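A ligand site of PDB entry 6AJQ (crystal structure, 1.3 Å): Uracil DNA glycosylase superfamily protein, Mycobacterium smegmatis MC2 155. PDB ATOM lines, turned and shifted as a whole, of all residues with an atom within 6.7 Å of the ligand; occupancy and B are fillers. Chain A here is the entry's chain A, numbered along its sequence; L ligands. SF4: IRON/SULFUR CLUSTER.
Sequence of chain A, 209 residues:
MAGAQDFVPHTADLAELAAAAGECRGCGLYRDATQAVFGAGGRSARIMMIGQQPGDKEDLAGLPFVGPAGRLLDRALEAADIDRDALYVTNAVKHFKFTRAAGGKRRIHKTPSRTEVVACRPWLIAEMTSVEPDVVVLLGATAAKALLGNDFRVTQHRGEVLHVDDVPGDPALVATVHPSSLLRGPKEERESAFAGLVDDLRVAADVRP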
ATOM      1  N   GLY A   3      14.842   6.355  15.397  1.00  0.00           N
ATOM      2  CA  GLY A   3      15.687   6.705  16.540  1.00  0.00           C
ATOM      3  C   GLY A   3      14.958   7.468  17.623  1.00  0.00           C
ATOM      4  O   GLY A   3      13.826   7.147  18.020  1.00  0.00           O
ATOM      5  N   ALA A   4      15.621   8.506  18.138  1.00  0.00           N
ATOM      6  CA  ALA A   4      15.130   9.317  19.240  1.00  0.00           C
ATOM      7  C   ALA A   4      14.128  10.387  18.795  1.00  0.00           C
ATOM      8  O   ALA A   4      13.602  11.086  19.649  1.00  0.00           O
ATOM      9  CB  ALA A   4      16.313  10.001  19.944  1.00  0.00           C
ATOM     10  N   PHE A   7      10.903  11.311  20.575  1.00  0.00           N
ATOM     11  CA  PHE A   7      11.032  11.656  21.973  1.00  0.00           C
ATOM     12  C   PHE A   7      11.468  13.105  22.184  1.00  0.00           C
ATOM     13  O   PHE A   7      11.381  13.589  23.312  1.00  0.00           O
ATOM     14  CB  PHE A   7      12.001  10.691  22.663  1.00  0.00           C
ATOM     15  CG  PHE A   7      11.517   9.257  22.685  1.00  0.00           C
ATOM     16  CD1 PHE A   7      10.608   8.853  23.639  1.00  0.00           C
ATOM     17  CD2 PHE A   7      11.942   8.352  21.740  1.00  0.00           C
ATOM     18  CE1 PHE A   7      10.128   7.537  23.668  1.00  0.00           C
ATOM     19  CE2 PHE A   7      11.460   7.027  21.765  1.00  0.00           C
ATOM     20  CZ  PHE A   7      10.563   6.645  22.741  1.00  0.00           C
ATOM     21  N   ALA A  21      14.613  13.751  27.555  1.00  0.00           N
ATOM     22  CA  ALA A  21      15.607  12.715  27.278  1.00  0.00           C
ATOM     23  C   ALA A  21      15.592  11.628  28.337  1.00  0.00           C
ATOM     24  O   ALA A  21      15.927  10.482  28.056  1.00  0.00           O
ATOM     25  CB  ALA A  21      17.005  13.306  27.094  1.00  0.00           C
ATOM     26  N   GLU A  23      13.122  10.179  29.301  1.00  0.00           N
ATOM     27  CA  GLU A  23      12.119   9.229  28.845  1.00  0.00           C
ATOM     28  C   GLU A  23      12.469   8.555  27.520  1.00  0.00           C
ATOM     29  O   GLU A  23      11.673   7.776  27.013  1.00  0.00           O
ATOM     30  CB  GLU A  23      10.753   9.926  28.706  1.00  0.00           C
ATOM     31  CG  GLU A  23      10.216  10.580  29.972  1.00  0.00           C
ATOM     32  CD  GLU A  23      10.329   9.698  31.188  1.00  0.00           C
ATOM     33  OE1 GLU A  23      10.970  10.105  32.171  1.00  0.00           O
ATOM     34  OE2 GLU A  23       9.754   8.580  31.163  1.00  0.00           O
ATOM     35  N   CYS A  24      13.621   8.846  26.942  1.00  0.00           N
ATOM     36  CA  CYS A  24      13.918   8.364  25.609  1.00  0.00           C
ATOM     37  C   CYS A  24      14.123   6.847  25.602  1.00  0.00           C
ATOM     38  O   CYS A  24      14.760   6.287  26.493  1.00  0.00           O
ATOM     39  CB  CYS A  24      15.201   9.031  25.091  1.00  0.00           C
ATOM     40  SG  CYS A  24      15.539   8.635  23.367  1.00  0.00           S
ATOM     41  N   ARG A  25      13.547   6.192  24.591  1.00  0.00           N
ATOM     42  CA  ARG A  25      13.820   4.793  24.315  1.00  0.00           C
ATOM     43  C   ARG A  25      14.302   4.610  22.878  1.00  0.00           C
ATOM     44  O   ARG A  25      14.101   3.544  22.277  1.00  0.00           O
ATOM     45  CB  ARG A  25      12.579   3.933  24.606  1.00  0.00           C
ATOM     46  CG  ARG A  25      12.068   4.026  26.037  1.00  0.00           C
ATOM     47  CD  ARG A  25      10.915   3.009  26.282  1.00  0.00           C
ATOM     48  NE  ARG A  25       9.993   2.952  25.145  1.00  0.00           N
ATOM     49  CZ  ARG A  25       9.023   3.841  24.960  1.00  0.00           C
ATOM     50  NH1 ARG A  25       8.885   4.844  25.825  1.00  0.00           N
ATOM     51  NH2 ARG A  25       8.207   3.751  23.924  1.00  0.00           N
ATOM     52  N   GLY A  26      14.937   5.635  22.316  1.00  0.00           N
ATOM     53  CA  GLY A  26      15.237   5.696  20.899  1.00  0.00           C
ATOM     54  C   GLY A  26      16.181   4.618  20.403  1.00  0.00           C
ATOM     55  O   GLY A  26      16.244   4.369  19.201  1.00  0.00           O
ATOM     56  N   CYS A  27      16.930   3.982  21.306  1.00  0.00           N
ATOM     57  CA  CYS A  27      17.752   2.823  20.996  1.00  0.00           C
ATOM     58  C   CYS A  27      17.715   1.917  22.220  1.00  0.00           C
ATOM     59  O   CYS A  27      16.965   2.156  23.165  1.00  0.00           O
ATOM     60  CB  CYS A  27      19.160   3.204  20.513  1.00  0.00           C
ATOM     61  SG  CYS A  27      20.324   3.715  21.807  1.00  0.00           S
ATOM     62  N   GLY A  28      18.527   0.869  22.209  1.00  0.00           N
ATOM     63  CA  GLY A  28      18.446  -0.049  23.325  1.00  0.00           C
ATOM     64  C   GLY A  28      19.199   0.382  24.564  1.00  0.00           C
ATOM     65  O   GLY A  28      19.063  -0.261  25.609  1.00  0.00           O
ATOM     66  N   LEU A  29      19.975   1.451  24.486  1.00  0.00           N
ATOM     67  CA  LEU A  29      20.912   1.773  25.562  1.00  0.00           C
ATOM     68  C   LEU A  29      20.220   2.225  26.842  1.00  0.00           C
ATOM     69  O   LEU A  29      20.810   2.117  27.923  1.00  0.00           O
ATOM     70  CB  LEU A  29      21.920   2.824  25.102  1.00  0.00           C
ATOM     71  CG  LEU A  29      22.821   2.326  23.977  1.00  0.00           C
ATOM     72  CD1 LEU A  29      23.796   3.403  23.603  1.00  0.00           C
ATOM     73  CD2 LEU A  29      23.522   1.006  24.392  1.00  0.00           C
ATOM     74  N   TYR A  30      18.976   2.713  26.763  1.00  0.00           N
ATOM     75  CA  TYR A  30      18.310   3.138  27.987  1.00  0.00           C
ATOM     76  C   TYR A  30      18.089   2.004  28.983  1.00  0.00           C
ATOM     77  O   TYR A  30      17.932   2.256  30.177  1.00  0.00           O
ATOM     78  CB  TYR A  30      16.943   3.790  27.689  1.00  0.00           C
ATOM     79  CG  TYR A  30      15.865   2.777  27.374  1.00  0.00           C
ATOM     80  CD1 TYR A  30      15.749   2.257  26.099  1.00  0.00           C
ATOM     81  CD2 TYR A  30      14.981   2.334  28.356  1.00  0.00           C
ATOM     82  CE1 TYR A  30      14.785   1.328  25.784  1.00  0.00           C
ATOM     83  CE2 TYR A  30      14.002   1.396  28.045  1.00  0.00           C
ATOM     84  CZ  TYR A  30      13.919   0.906  26.758  1.00  0.00           C
ATOM     85  OH  TYR A  30      12.956  -0.029  26.430  1.00  0.00           O
ATOM     86  N   ARG A  31      18.066   0.753  28.513  1.00  0.00           N
ATOM     87  CA  ARG A  31      17.601  -0.341  29.363  1.00  0.00           C
ATOM     88  C   ARG A  31      18.552  -0.610  30.523  1.00  0.00           C
ATOM     89  O   ARG A  31      18.120  -0.731  31.677  1.00  0.00           O
ATOM     90  CB  ARG A  31      17.400  -1.600  28.531  1.00  0.00           C
ATOM     91  CG  ARG A  31      16.267  -1.512  27.537  1.00  0.00           C
ATOM     92  CD  ARG A  31      15.861  -2.909  27.077  1.00  0.00           C
ATOM     93  NE  ARG A  31      15.676  -2.973  25.621  1.00  0.00           N
ATOM     94  CZ  ARG A  31      16.685  -3.086  24.761  1.00  0.00           C
ATOM     95  NH1 ARG A  31      16.436  -3.135  23.465  1.00  0.00           N
ATOM     96  NH2 ARG A  31      17.931  -3.156  25.191  1.00  0.00           N
ATOM     97  N   ALA A  36      19.439   8.770  31.589  1.00  0.00           N
ATOM     98  CA  ALA A  36      20.007   9.572  30.532  1.00  0.00           C
ATOM     99  C   ALA A  36      20.868  10.664  31.154  1.00  0.00           C
ATOM    100  O   ALA A  36      20.568  11.166  32.250  1.00  0.00           O
ATOM    101  CB  ALA A  36      18.895  10.205  29.705  1.00  0.00           C
ATOM    102  N   ALA A  92      27.770  12.333  22.381  1.00  0.00           N
ATOM    103  CA  ALA A  92      27.072  11.923  21.168  1.00  0.00           C
ATOM    104  C   ALA A  92      25.920  10.982  21.472  1.00  0.00           C
ATOM    105  O   ALA A  92      24.876  11.039  20.797  1.00  0.00           O
ATOM    106  CB  ALA A  92      28.067  11.262  20.197  1.00  0.00           C
ATOM    107  N   VAL A  93      26.075  10.112  22.473  1.00  0.00           N
ATOM    108  CA  VAL A  93      24.954   9.308  22.934  1.00  0.00           C
ATOM    109  C   VAL A  93      24.786   9.590  24.411  1.00  0.00           C
ATOM    110  O   VAL A  93      25.724   9.988  25.115  1.00  0.00           O
ATOM    111  CB  VAL A  93      25.037   7.795  22.666  1.00  0.00           C
ATOM    112  CG1 VAL A  93      25.270   7.504  21.176  1.00  0.00           C
ATOM    113  CG2 VAL A  93      26.086   7.134  23.541  1.00  0.00           C
ATOM    114  N   LYS A  94      23.543   9.436  24.870  1.00  0.00           N
ATOM    115  CA  LYS A  94      23.198   9.956  26.190  1.00  0.00           C
ATOM    116  C   LYS A  94      22.922   8.882  27.232  1.00  0.00           C
ATOM    117  O   LYS A  94      22.601   9.225  28.379  1.00  0.00           O
ATOM    118  CB  LYS A  94      22.082  10.987  26.092  1.00  0.00           C
ATOM    119  CG  LYS A  94      22.600  12.151  25.206  1.00  0.00           C
ATOM    120  CD  LYS A  94      21.645  13.281  25.018  1.00  0.00           C
ATOM    121  CE  LYS A  94      22.437  14.552  24.736  1.00  0.00           C
ATOM    122  NZ  LYS A  94      23.311  14.524  23.505  1.00  0.00           N
ATOM    123  N   HIS A  95      23.112   7.616  26.895  1.00  0.00           N
ATOM    124  CA  HIS A  95      23.063   6.529  27.866  1.00  0.00           C
ATOM    125  C   HIS A  95      24.368   5.740  27.809  1.00  0.00           C
ATOM    126  O   HIS A  95      24.913   5.505  26.730  1.00  0.00           O
ATOM    127  CB  HIS A  95      21.886   5.595  27.577  1.00  0.00           C
ATOM    128  CG  HIS A  95      20.567   6.085  28.072  1.00  0.00           C
ATOM    129  ND1 HIS A  95      19.597   6.589  27.238  1.00  0.00           N
ATOM    130  CD2 HIS A  95      20.032   6.106  29.315  1.00  0.00           C
ATOM    131  CE1 HIS A  95      18.539   6.934  27.938  1.00  0.00           C
ATOM    132  NE2 HIS A  95      18.761   6.615  29.201  1.00  0.00           N
ATOM    133  N   PHE A  96      24.845   5.345  28.978  1.00  0.00           N
ATOM    134  CA  PHE A  96      26.101   4.615  29.124  1.00  0.00           C
ATOM    135  C   PHE A  96      25.927   3.178  28.629  1.00  0.00           C
ATOM    136  O   PHE A  96      25.046   2.459  29.099  1.00  0.00           O
ATOM    137  CB  PHE A  96      26.420   4.622  30.617  1.00  0.00           C
ATOM    138  CG  PHE A  96      27.683   3.901  31.034  1.00  0.00           C
ATOM    139  CD1 PHE A  96      28.851   3.933  30.298  1.00  0.00           C
ATOM    140  CD2 PHE A  96      27.702   3.281  32.283  1.00  0.00           C
ATOM    141  CE1 PHE A  96      30.011   3.293  30.763  1.00  0.00           C
ATOM    142  CE2 PHE A  96      28.843   2.648  32.744  1.00  0.00           C
ATOM    143  CZ  PHE A  96      29.983   2.656  32.001  1.00  0.00           C
ATOM    144  N   GLU A 116      23.436   3.347  16.921  1.00  0.00           N
ATOM    145  CA  GLU A 116      23.103   4.069  18.146  1.00  0.00           C
ATOM    146  C   GLU A 116      23.431   5.561  18.047  1.00  0.00           C
ATOM    147  O   GLU A 116      22.642   6.410  18.474  1.00  0.00           O
ATOM    148  CB  GLU A 116      23.801   3.421  19.349  1.00  0.00           C
ATOM    149  CG  GLU A 116      23.216   2.032  19.640  1.00  0.00           C
ATOM    150  CD  GLU A 116      24.155   1.121  20.404  1.00  0.00           C
ATOM    151  OE1 GLU A 116      25.393   1.327  20.414  1.00  0.00           O
ATOM    152  OE2 GLU A 116      23.629   0.151  20.987  1.00  0.00           O
ATOM    153  N   ALA A 119      20.776   7.092  15.971  1.00  0.00           N
ATOM    154  CA  ALA A 119      19.517   7.121  16.719  1.00  0.00           C
ATOM    155  C   ALA A 119      19.470   8.287  17.701  1.00  0.00           C
ATOM    156  O   ALA A 119      18.417   8.892  17.903  1.00  0.00           O
ATOM    157  CB  ALA A 119      19.290   5.800  17.474  1.00  0.00           C
ATOM    158  N   CYS A 120      20.592   8.585  18.356  1.00  0.00           N
ATOM    159  CA  CYS A 120      20.630   9.594  19.403  1.00  0.00           C
ATOM    160  C   CYS A 120      20.869  10.987  18.843  1.00  0.00           C
ATOM    161  O   CYS A 120      20.639  11.991  19.544  1.00  0.00           O
ATOM    162  CB  CYS A 120      21.728   9.249  20.422  1.00  0.00           C
ATOM    163  SG  CYS A 120      21.462   9.953  22.084  1.00  0.00           S
ATOM    164  N   ARG A 121      21.305  11.090  17.596  1.00  0.00           N
ATOM    165  CA  ARG A 121      21.680  12.375  17.034  1.00  0.00           C
ATOM    166  C   ARG A 121      20.560  13.417  17.071  1.00  0.00           C
ATOM    167  O   ARG A 121      20.894  14.619  17.187  1.00  0.00           O
ATOM    168  CB  ARG A 121      22.221  12.182  15.613  1.00  0.00           C
ATOM    169  CG  ARG A 121      23.035  13.378  15.125  1.00  0.00           C
ATOM    170  CD  ARG A 121      23.858  13.049  13.875  1.00  0.00           C
ATOM    171  NE  ARG A 121      23.037  12.458  12.848  1.00  0.00           N
ATOM    172  CZ  ARG A 121      23.514  11.753  11.821  1.00  0.00           C
ATOM    173  NH1 ARG A 121      24.822  11.560  11.710  1.00  0.00           N
ATOM    174  NH2 ARG A 121      22.700  11.240  10.922  1.00  0.00           N
ATOM    175  N   PRO A 122      19.277  13.076  17.013  1.00  0.00           N
ATOM    176  CA  PRO A 122      18.260  14.137  17.190  1.00  0.00           C
ATOM    177  C   PRO A 122      18.450  14.949  18.467  1.00  0.00           C
ATOM    178  O   PRO A 122      18.131  16.149  18.473  1.00  0.00           O
ATOM    179  CB  PRO A 122      16.941  13.347  17.168  1.00  0.00           C
ATOM    180  CG  PRO A 122      17.227  12.225  16.237  1.00  0.00           C
ATOM    181  CD  PRO A 122      18.668  11.827  16.522  1.00  0.00           C
ATOM    182  N   TRP A 123      18.927  14.340  19.564  1.00  0.00           N
ATOM    183  CA  TRP A 123      19.194  15.134  20.761  1.00  0.00           C
ATOM    184  C   TRP A 123      20.333  16.109  20.518  1.00  0.00           C
ATOM    185  O   TRP A 123      20.243  17.275  20.933  1.00  0.00           O
ATOM    186  CB  TRP A 123      19.517  14.221  21.959  1.00  0.00           C
ATOM    187  CG  TRP A 123      18.352  13.391  22.429  1.00  0.00           C
ATOM    188  CD1 TRP A 123      18.251  12.028  22.382  1.00  0.00           C
ATOM    189  CD2 TRP A 123      17.120  13.866  22.992  1.00  0.00           C
ATOM    190  NE1 TRP A 123      17.035  11.626  22.890  1.00  0.00           N
ATOM    191  CE2 TRP A 123      16.324  12.743  23.267  1.00  0.00           C
ATOM    192  CE3 TRP A 123      16.609  15.145  23.292  1.00  0.00           C
ATOM    193  CZ2 TRP A 123      15.041  12.851  23.812  1.00  0.00           C
ATOM    194  CZ3 TRP A 123      15.356  15.247  23.834  1.00  0.00           C
ATOM    195  CH2 TRP A 123      14.589  14.109  24.102  1.00  0.00           C
HETATM  196 FE1  SF4 L   1      17.623   7.608  23.471  1.00  0.00          FE
HETATM  197 FE2  SF4 L   1      20.170   8.318  22.995  1.00  0.00          FE
HETATM  198 FE3  SF4 L   1      19.477   5.709  22.764  1.00  0.00          FE
HETATM  199 FE4  SF4 L   1      19.532   6.860  25.171  1.00  0.00          FE
HETATM  200  S1  SF4 L   1      21.357   6.535  23.828  1.00  0.00           S
HETATM  201  S2  SF4 L   1      17.811   5.520  24.375  1.00  0.00           S
HETATM  202  S3  SF4 L   1      18.887   9.015  24.766  1.00  0.00           S
HETATM  203  S4  SF4 L   1      18.701   7.400  21.463  1.00  0.00           S
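N of His 95 sits close to S1 of the ligand, at 3.7 Å. A ring nitrogen (ND1) of His 95 is bound to an iron atom (FE4) of the ligand (2.1 Å). The side-chain sulfur (SG) of Cys 120 binds an iron atom (FE2) of the ligand, 2.3 Å away. An iron atom (FE1) of the ligand is bound by the side-chain sulfur (SG) of Cys 24. The backbone NH (N) of Cys 27 lies close to a sulfur (S2) of the ligand (3.5 Å). The side-chain sulfur of Cys 27 is bound to an iron atom (FE3) of the ligand. A sulfur (S2) of the ligand sits close to the backbone NH (N) of Gly 26. The indole nitrogen of Trp 123 sits close to a sulfur (S3) of the ligand, 3.7 Å away. A sulfur (S1) of the ligand lies close to the backbone NH of Lys 94, at 3.8 Å.
The backbone NH (N) of Ala 36 is in hydrogen-bond range of a ring nitrogen (NE2) of His 95 (3.3 Å). SG of Cys 120 sits close to N of Lys 94 (3.5 Å). The side-chain sulfur (SG) of Cys 24 lies close to the backbone NH (N) of Gly 26, 3.2 Å away. SG of Cys 24 lies close to NE1 of Trp 123 (3.4 Å). The backbone NH (N) of Leu 29 lies close to the side-chain sulfur (SG) of Cys 27 (3.5 Å). The backbone NH (N) of Ala 4 sits at hydrogen-bond distance from the backbone carbonyl oxygen (O) of Ala 119.
Ala 4 touches the ligand (CB to S4, 3.8 Å). C of Arg 25 touches S2 of the ligand (3.9 Å). Leu 29 touches the ligand (CB to S1, 3.96 Å). CB of Tyr 30 touches S2 of the ligand, at 3.8 Å. Ala 119 touches the ligand. Hydrophobic or aromatic side chains that line the ligand: Ala 4, Leu 29, Tyr 30, His 95 and Trp 123. Within 4 Å of the ligand: Ala 4, Cys 24, Arg 25, Gly 26, Cys 27, Leu 29, Tyr 30, Lys 94, His 95, Ala 119, Cys 120 and Trp 123.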
